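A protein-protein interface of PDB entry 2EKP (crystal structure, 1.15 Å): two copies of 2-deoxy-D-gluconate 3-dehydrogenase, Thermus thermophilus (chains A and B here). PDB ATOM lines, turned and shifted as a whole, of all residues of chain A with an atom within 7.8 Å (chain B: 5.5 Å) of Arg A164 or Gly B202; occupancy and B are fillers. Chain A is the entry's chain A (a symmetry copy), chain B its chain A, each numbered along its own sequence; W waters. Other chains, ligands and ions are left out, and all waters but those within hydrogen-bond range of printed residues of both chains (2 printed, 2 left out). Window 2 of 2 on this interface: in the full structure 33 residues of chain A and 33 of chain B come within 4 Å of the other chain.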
ATOM      1  N   ALA A 117     -31.727  27.954   3.495  1.00  0.00           N
ATOM      2  CA  ALA A 117     -32.391  26.710   3.127  1.00  0.00           C
ATOM      3  C   ALA A 117     -33.205  26.880   1.845  1.00  0.00           C
ATOM      4  O   ALA A 117     -33.192  26.010   0.977  1.00  0.00           O
ATOM      5  CB  ALA A 117     -33.283  26.237   4.265  1.00  0.00           C
ATOM      6  N   GLY A 120     -31.049  26.664  -0.873  1.00  0.00           N
ATOM      7  CA  GLY A 120     -30.406  25.364  -0.958  1.00  0.00           C
ATOM      8  C   GLY A 120     -28.899  25.450  -0.787  1.00  0.00           C
ATOM      9  O   GLY A 120     -28.177  24.506  -1.107  1.00  0.00           O
ATOM     10  N   LEU A 158     -25.382  23.276  15.170  1.00  0.00           N
ATOM     11  CA  LEU A 158     -26.081  23.797  14.003  1.00  0.00           C
ATOM     12  C   LEU A 158     -25.617  23.111  12.723  1.00  0.00           C
ATOM     13  O   LEU A 158     -26.416  22.870  11.816  1.00  0.00           O
ATOM     14  CB  LEU A 158     -25.893  25.312  13.891  1.00  0.00           C
ATOM     15  CG  LEU A 158     -26.388  26.133  15.086  1.00  0.00           C
ATOM     16  CD1 LEU A 158     -26.260  27.614  14.768  1.00  0.00           C
ATOM     17  CD2 LEU A 158     -27.836  25.782  15.408  1.00  0.00           C
ATOM     18  N   ALA A 159     -24.329  22.795  12.646  1.00  0.00           N
ATOM     19  CA  ALA A 159     -23.807  22.107  11.474  1.00  0.00           C
ATOM     20  C   ALA A 159     -24.520  20.765  11.316  1.00  0.00           C
ATOM     21  O   ALA A 159     -24.918  20.381  10.214  1.00  0.00           O
ATOM     22  CB  ALA A 159     -22.309  21.882  11.624  1.00  0.00           C
ATOM     23  N   LYS A 160     -24.681  20.048  12.424  1.00  0.00           N
ATOM     24  CA  LYS A 160     -25.332  18.745  12.385  1.00  0.00           C
ATOM     25  C   LYS A 160     -26.776  18.844  11.908  1.00  0.00           C
ATOM     26  O   LYS A 160     -27.212  18.069  11.057  1.00  0.00           O
ATOM     27  CB  LYS A 160     -25.315  18.087  13.767  1.00  0.00           C
ATOM     28  CG  LYS A 160     -25.953  16.700  13.766  1.00  0.00           C
ATOM     29  CD  LYS A 160     -26.178  16.139  15.164  1.00  0.00           C
ATOM     30  CE  LYS A 160     -27.209  16.945  15.937  1.00  0.00           C
ATOM     31  NZ  LYS A 160     -27.571  16.302  17.234  1.00  0.00           N
ATOM     32  N   GLU A 161     -27.515  19.801  12.456  1.00  0.00           N
ATOM     33  CA  GLU A 161     -28.916  19.949  12.095  1.00  0.00           C
ATOM     34  C   GLU A 161     -29.207  20.516  10.721  1.00  0.00           C
ATOM     35  O   GLU A 161     -30.221  20.178  10.115  1.00  0.00           O
ATOM     36  CB  GLU A 161     -29.645  20.813  13.125  1.00  0.00           C
ATOM     37  CG  GLU A 161     -29.487  20.336  14.548  1.00  0.00           C
ATOM     38  CD  GLU A 161     -30.489  20.958  15.496  1.00  0.00           C
ATOM     39  OE1 GLU A 161     -31.005  22.059  15.200  1.00  0.00           O
ATOM     40  OE2 GLU A 161     -30.748  20.339  16.552  1.00  0.00           O
ATOM     41  N   TRP A 162     -28.327  21.371  10.217  1.00  0.00           N
ATOM     42  CA  TRP A 162     -28.594  22.015   8.937  1.00  0.00           C
ATOM     43  C   TRP A 162     -27.825  21.512   7.724  1.00  0.00           C
ATOM     44  O   TRP A 162     -27.996  22.030   6.619  1.00  0.00           O
ATOM     45  CB  TRP A 162     -28.392  23.528   9.084  1.00  0.00           C
ATOM     46  CG  TRP A 162     -29.240  24.142  10.167  1.00  0.00           C
ATOM     47  CD1 TRP A 162     -30.367  23.612  10.729  1.00  0.00           C
ATOM     48  CD2 TRP A 162     -29.042  25.415  10.795  1.00  0.00           C
ATOM     49  NE1 TRP A 162     -30.883  24.474  11.669  1.00  0.00           N
ATOM     50  CE2 TRP A 162     -30.090  25.590  11.727  1.00  0.00           C
ATOM     51  CE3 TRP A 162     -28.083  26.425  10.658  1.00  0.00           C
ATOM     52  CZ2 TRP A 162     -30.202  26.738  12.522  1.00  0.00           C
ATOM     53  CZ3 TRP A 162     -28.195  27.566  11.448  1.00  0.00           C
ATOM     54  CH2 TRP A 162     -29.249  27.712  12.366  1.00  0.00           C
ATOM     55  N   ALA A 163     -26.994  20.495   7.917  1.00  0.00           N
ATOM     56  CA  ALA A 163     -26.199  19.946   6.822  1.00  0.00           C
ATOM     57  C   ALA A 163     -27.041  19.558   5.607  1.00  0.00           C
ATOM     58  O   ALA A 163     -26.701  19.910   4.475  1.00  0.00           O
ATOM     59  CB  ALA A 163     -25.419  18.731   7.314  1.00  0.00           C
ATOM     60  N   ARG A 164     -28.140  18.844   5.839  1.00  0.00           N
ATOM     61  CA  ARG A 164     -28.985  18.395   4.739  1.00  0.00           C
ATOM     62  C   ARG A 164     -29.700  19.541   4.020  1.00  0.00           C
ATOM     63  O   ARG A 164     -30.241  19.347   2.928  1.00  0.00           O
ATOM     64  CB  ARG A 164     -30.018  17.385   5.248  1.00  0.00           C
ATOM     65  CG  ARG A 164     -29.468  16.091   5.903  1.00  0.00           C
ATOM     66  CD  ARG A 164     -28.647  15.238   4.938  1.00  0.00           C
ATOM     67  NE  ARG A 164     -28.458  13.851   5.356  1.00  0.00           N
ATOM     68  CZ  ARG A 164     -29.216  12.829   4.953  1.00  0.00           C
ATOM     69  NH1 ARG A 164     -30.229  13.027   4.112  1.00  0.00           N
ATOM     70  NH2 ARG A 164     -28.961  11.597   5.388  1.00  0.00           N
ATOM     71  N   LEU A 165     -29.711  20.725   4.632  1.00  0.00           N
ATOM     72  CA  LEU A 165     -30.356  21.889   4.027  1.00  0.00           C
ATOM     73  C   LEU A 165     -29.403  22.639   3.100  1.00  0.00           C
ATOM     74  O   LEU A 165     -29.786  23.627   2.465  1.00  0.00           O
ATOM     75  CB  LEU A 165     -30.869  22.845   5.106  1.00  0.00           C
ATOM     76  CG  LEU A 165     -31.881  22.289   6.112  1.00  0.00           C
ATOM     77  CD1 LEU A 165     -32.218  23.354   7.143  1.00  0.00           C
ATOM     78  CD2 LEU A 165     -33.138  21.827   5.387  1.00  0.00           C
ATOM     79  N   GLY A 166     -28.160  22.169   3.029  1.00  0.00           N
ATOM     80  CA  GLY A 166     -27.166  22.809   2.185  1.00  0.00           C
ATOM     81  C   GLY A 166     -26.375  23.883   2.906  1.00  0.00           C
ATOM     82  O   GLY A 166     -25.608  24.618   2.289  1.00  0.00           O
ATOM     83  N   ILE A 167     -26.553  23.970   4.219  1.00  0.00           N
ATOM     84  CA  ILE A 167     -25.867  24.967   5.027  1.00  0.00           C
ATOM     85  C   ILE A 167     -24.638  24.377   5.706  1.00  0.00           C
ATOM     86  O   ILE A 167     -24.685  23.265   6.227  1.00  0.00           O
ATOM     87  CB  ILE A 167     -26.811  25.524   6.126  1.00  0.00           C
ATOM     88  CG1 ILE A 167     -28.064  26.120   5.481  1.00  0.00           C
ATOM     89  CG2 ILE A 167     -26.088  26.572   6.964  1.00  0.00           C
ATOM     90  CD1 ILE A 167     -29.120  26.568   6.472  1.00  0.00           C
ATOM     91  N   ARG A 168     -23.535  25.117   5.670  1.00  0.00           N
ATOM     92  CA  ARG A 168     -22.308  24.701   6.334  1.00  0.00           C
ATOM     93  C   ARG A 168     -22.104  25.715   7.463  1.00  0.00           C
ATOM     94  O   ARG A 168     -22.328  26.916   7.274  1.00  0.00           O
ATOM     95  CB  ARG A 168     -21.125  24.727   5.363  1.00  0.00           C
ATOM     96  CG  ARG A 168     -21.373  23.962   4.068  1.00  0.00           C
ATOM     97  CD  ARG A 168     -21.588  22.470   4.297  1.00  0.00           C
ATOM     98  NE  ARG A 168     -22.058  21.805   3.082  1.00  0.00           N
ATOM     99  CZ  ARG A 168     -23.286  21.324   2.913  1.00  0.00           C
ATOM    100  NH1 ARG A 168     -24.189  21.424   3.880  1.00  0.00           N
ATOM    101  NH2 ARG A 168     -23.613  20.732   1.771  1.00  0.00           N
ATOM    102  N   TYR A 224     -17.788  20.417   1.623  1.00  0.00           N
ATOM    103  CA  TYR A 224     -17.790  19.237   2.486  1.00  0.00           C
ATOM    104  C   TYR A 224     -17.136  19.533   3.839  1.00  0.00           C
ATOM    105  O   TYR A 224     -16.738  18.613   4.557  1.00  0.00           O
ATOM    106  CB  TYR A 224     -17.057  18.072   1.799  1.00  0.00           C
ATOM    107  CG  TYR A 224     -17.500  16.698   2.263  1.00  0.00           C
ATOM    108  CD1 TYR A 224     -18.738  16.184   1.885  1.00  0.00           C
ATOM    109  CD2 TYR A 224     -16.687  15.917   3.086  1.00  0.00           C
ATOM    110  CE1 TYR A 224     -19.163  14.929   2.315  1.00  0.00           C
ATOM    111  CE2 TYR A 224     -17.103  14.657   3.525  1.00  0.00           C
ATOM    112  CZ  TYR A 224     -18.340  14.170   3.136  1.00  0.00           C
ATOM    113  OH  TYR A 224     -18.748  12.928   3.575  1.00  0.00           O
ATOM    114  N   THR B 196     -22.081   6.077   7.682  1.00  0.00           N
ATOM    115  CA  THR B 196     -22.803   7.095   6.941  1.00  0.00           C
ATOM    116  C   THR B 196     -23.924   7.729   7.760  1.00  0.00           C
ATOM    117  O   THR B 196     -24.257   8.897   7.564  1.00  0.00           O
ATOM    118  CB  THR B 196     -23.350   6.510   5.628  1.00  0.00           C
ATOM    119  OG1 THR B 196     -22.270   5.914   4.898  1.00  0.00           O
ATOM    120  CG2 THR B 196     -23.980   7.602   4.777  1.00  0.00           C
ATOM    121  N   ILE B 199     -22.784  10.884   9.294  1.00  0.00           N
ATOM    122  CA  ILE B 199     -22.350  11.993   8.447  1.00  0.00           C
ATOM    123  C   ILE B 199     -23.573  12.880   8.226  1.00  0.00           C
ATOM    124  O   ILE B 199     -24.490  12.504   7.495  1.00  0.00           O
ATOM    125  CB  ILE B 199     -21.849  11.510   7.066  1.00  0.00           C
ATOM    126  CG1 ILE B 199     -20.709  10.503   7.237  1.00  0.00           C
ATOM    127  CG2 ILE B 199     -21.386  12.707   6.236  1.00  0.00           C
ATOM    128  CD1 ILE B 199     -20.249   9.878   5.932  1.00  0.00           C
ATOM    129  N   PRO B 200     -23.610  14.063   8.859  1.00  0.00           N
ATOM    130  CA  PRO B 200     -24.751  14.972   8.701  1.00  0.00           C
ATOM    131  C   PRO B 200     -25.147  15.249   7.250  1.00  0.00           C
ATOM    132  O   PRO B 200     -26.335  15.316   6.929  1.00  0.00           O
ATOM    133  CB  PRO B 200     -24.290  16.227   9.435  1.00  0.00           C
ATOM    134  CG  PRO B 200     -23.469  15.657  10.555  1.00  0.00           C
ATOM    135  CD  PRO B 200     -22.650  14.598   9.843  1.00  0.00           C
ATOM    136  N   MET B 201     -24.163  15.413   6.372  1.00  0.00           N
ATOM    137  CA  MET B 201     -24.469  15.672   4.972  1.00  0.00           C
ATOM    138  C   MET B 201     -25.099  14.465   4.278  1.00  0.00           C
ATOM    139  O   MET B 201     -25.617  14.582   3.168  1.00  0.00           O
ATOM    140  CB  MET B 201     -23.218  16.145   4.230  1.00  0.00           C
ATOM    141  CG  MET B 201     -22.911  17.608   4.516  1.00  0.00           C
ATOM    142  SD  MET B 201     -21.488  18.274   3.643  1.00  0.00           S
ATOM    143  CE  MET B 201     -21.949  17.953   1.945  1.00  0.00           C
ATOM    144  N   GLY B 202     -25.048  13.308   4.934  1.00  0.00           N
ATOM    145  CA  GLY B 202     -25.671  12.110   4.396  1.00  0.00           C
ATOM    146  C   GLY B 202     -25.027  11.428   3.208  1.00  0.00           C
ATOM    147  O   GLY B 202     -25.642  10.559   2.590  1.00  0.00           O
ATOM    148  N   ARG B 203     -23.794  11.796   2.887  1.00  0.00           N
ATOM    149  CA  ARG B 203     -23.103  11.194   1.758  1.00  0.00           C
ATOM    150  C   ARG B 203     -21.606  11.288   1.961  1.00  0.00           C
ATOM    151  O   ARG B 203     -21.128  12.098   2.758  1.00  0.00           O
ATOM    152  CB  ARG B 203     -23.467  11.919   0.459  1.00  0.00           C
ATOM    153  CG  ARG B 203     -22.918  13.347   0.369  1.00  0.00           C
ATOM    154  CD  ARG B 203     -23.247  13.997  -0.970  1.00  0.00           C
ATOM    155  NE  ARG B 203     -22.808  15.389  -1.061  1.00  0.00           N
ATOM    156  CZ  ARG B 203     -21.551  15.782  -1.254  1.00  0.00           C
ATOM    157  NH1 ARG B 203     -20.577  14.891  -1.379  1.00  0.00           N
ATOM    158  NH2 ARG B 203     -21.271  17.076  -1.336  1.00  0.00           N
ATOM    159  N   TRP B 204     -20.877  10.451   1.233  1.00  0.00           N
ATOM    160  CA  TRP B 204     -19.427  10.449   1.280  1.00  0.00           C
ATOM    161  C   TRP B 204     -18.958  11.561   0.352  1.00  0.00           C
ATOM    162  O   TRP B 204     -19.723  12.053  -0.481  1.00  0.00           O
ATOM    163  CB  TRP B 204     -18.890   9.096   0.808  1.00  0.00           C
ATOM    164  CG  TRP B 204     -18.998   8.016   1.842  1.00  0.00           C
ATOM    165  CD1 TRP B 204     -20.010   7.837   2.744  1.00  0.00           C
ATOM    166  CD2 TRP B 204     -18.054   6.971   2.084  1.00  0.00           C
ATOM    167  NE1 TRP B 204     -19.748   6.745   3.536  1.00  0.00           N
ATOM    168  CE2 TRP B 204     -18.554   6.193   3.152  1.00  0.00           C
ATOM    169  CE3 TRP B 204     -16.831   6.613   1.501  1.00  0.00           C
ATOM    170  CZ2 TRP B 204     -17.871   5.080   3.653  1.00  0.00           C
ATOM    171  CZ3 TRP B 204     -16.151   5.505   1.999  1.00  0.00           C
ATOM    172  CH2 TRP B 204     -16.676   4.752   3.065  1.00  0.00           C
ATOM    173  N   GLY B 234     -17.840  16.438   6.092  1.00  0.00           N
ATOM    174  CA  GLY B 234     -19.288  16.476   5.980  1.00  0.00           C
ATOM    175  C   GLY B 234     -20.037  16.528   7.298  1.00  0.00           C
ATOM    176  O   GLY B 234     -21.247  16.291   7.343  1.00  0.00           O
HETATM  177  O   HOH W   1     -28.428  17.576   8.544  1.00  0.00           O
HETATM  178  O   HOH W   2     -26.643  10.438   7.429  1.00  0.00           O
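Of the 8 printed residues of chain B, 7 touch a printed residue of chain A.
Printed residues of chain B that touch a printed residue of chain A: Ile B199, Pro B200, Met B201, Gly B202, Arg B203, Trp B204 and Gly B234.
Along chain A the printed residues that touch a printed residue of chain B span positions 160 to 224.
Water W1 lies within hydrogen-bond range of the backbone carbonyl oxygen (O) of Lys A160 (2.8 Å), the backbone NH (N) of Arg A164 (3.0 Å), the backbone NH (N) of Ala A163 (3.3 Å) and the backbone carbonyl oxygen (O) of Pro B200 (3.5 Å).
Water W2 lies within hydrogen-bond range of O of Thr B196 (2.8 Å), O of Ile B199 (3.0 Å) and NH2 of Arg A164 (3.3 Å).
The backbone carbonyl oxygen (O) of Gly B234 lies within hydrogen-bond range of the backbone NH (N) of Met B201 (3.2 Å).
The side-chain hydroxyl (OG1) of Thr B196 lies within hydrogen-bond range of the indole nitrogen (NE1) of Trp B204, at 3.0 Å.
The backbone carbonyl oxygen (O) of Ala A163 sits at hydrogen-bond distance from the guanidinium group (NH1) of Arg A168 (3.0 Å).
CB of Pro B200 touches O of Lys A160, at 3.8 Å.
CB of Ala A163 touches CB of Pro B200, at 3.5 Å.
N of Met B201 touches CB of Ala A163, at 3.7 Å.
CD of Arg A164 touches O of Met B201, at 3.6 Å.
Ile B199 touches Tyr A224 (CG2 to OH, 3.8 Å).
Tyr A224 touches Met B201.
OH of Tyr A224 touches CA of Trp B204, at 3.4 Å.
No position is printed for both chains.
Gly B202 touches just one residue of chain A: Arg A164 (3.4 Å).
Of the printed residues of chain A, Met B201 touches Ala A163 (3.7 Å), Arg A164 (3.6 Å), Arg A168 (3.2 Å) and Tyr A224 (3.7 Å).
Printed residues of chain A within 4 Å of Trp B204: Tyr A224.
Glu A161 touches none of the printed residues of chain B.
Gly A120 touches none of the printed residues of chain B.
The nearest residue of chain B that does not touch Arg A164 is Ile B199 (4.7 Å).
The nearest printed residue of chain B that does not touch Ala A163 is Gly B234 (4.8 Å).
The side-chain hydroxyl of Tyr A224 lies within hydrogen-bond range of the backbone carbonyl oxygen of Arg B203, 2.6 Å away.
The side-chain sulfur of Met B201 lies close to the guanidinium group of Arg A168 (3.6 Å).
N of Gly B234 sits at hydrogen-bond distance from O of Tyr A224 (2.9 Å).
O of Pro B200 sits at hydrogen-bond distance from NE of Arg A164.
The guanidinium group (NE) of Arg A164 sits close to the backbone NH (N) of Gly B202, at 3.5 Å.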
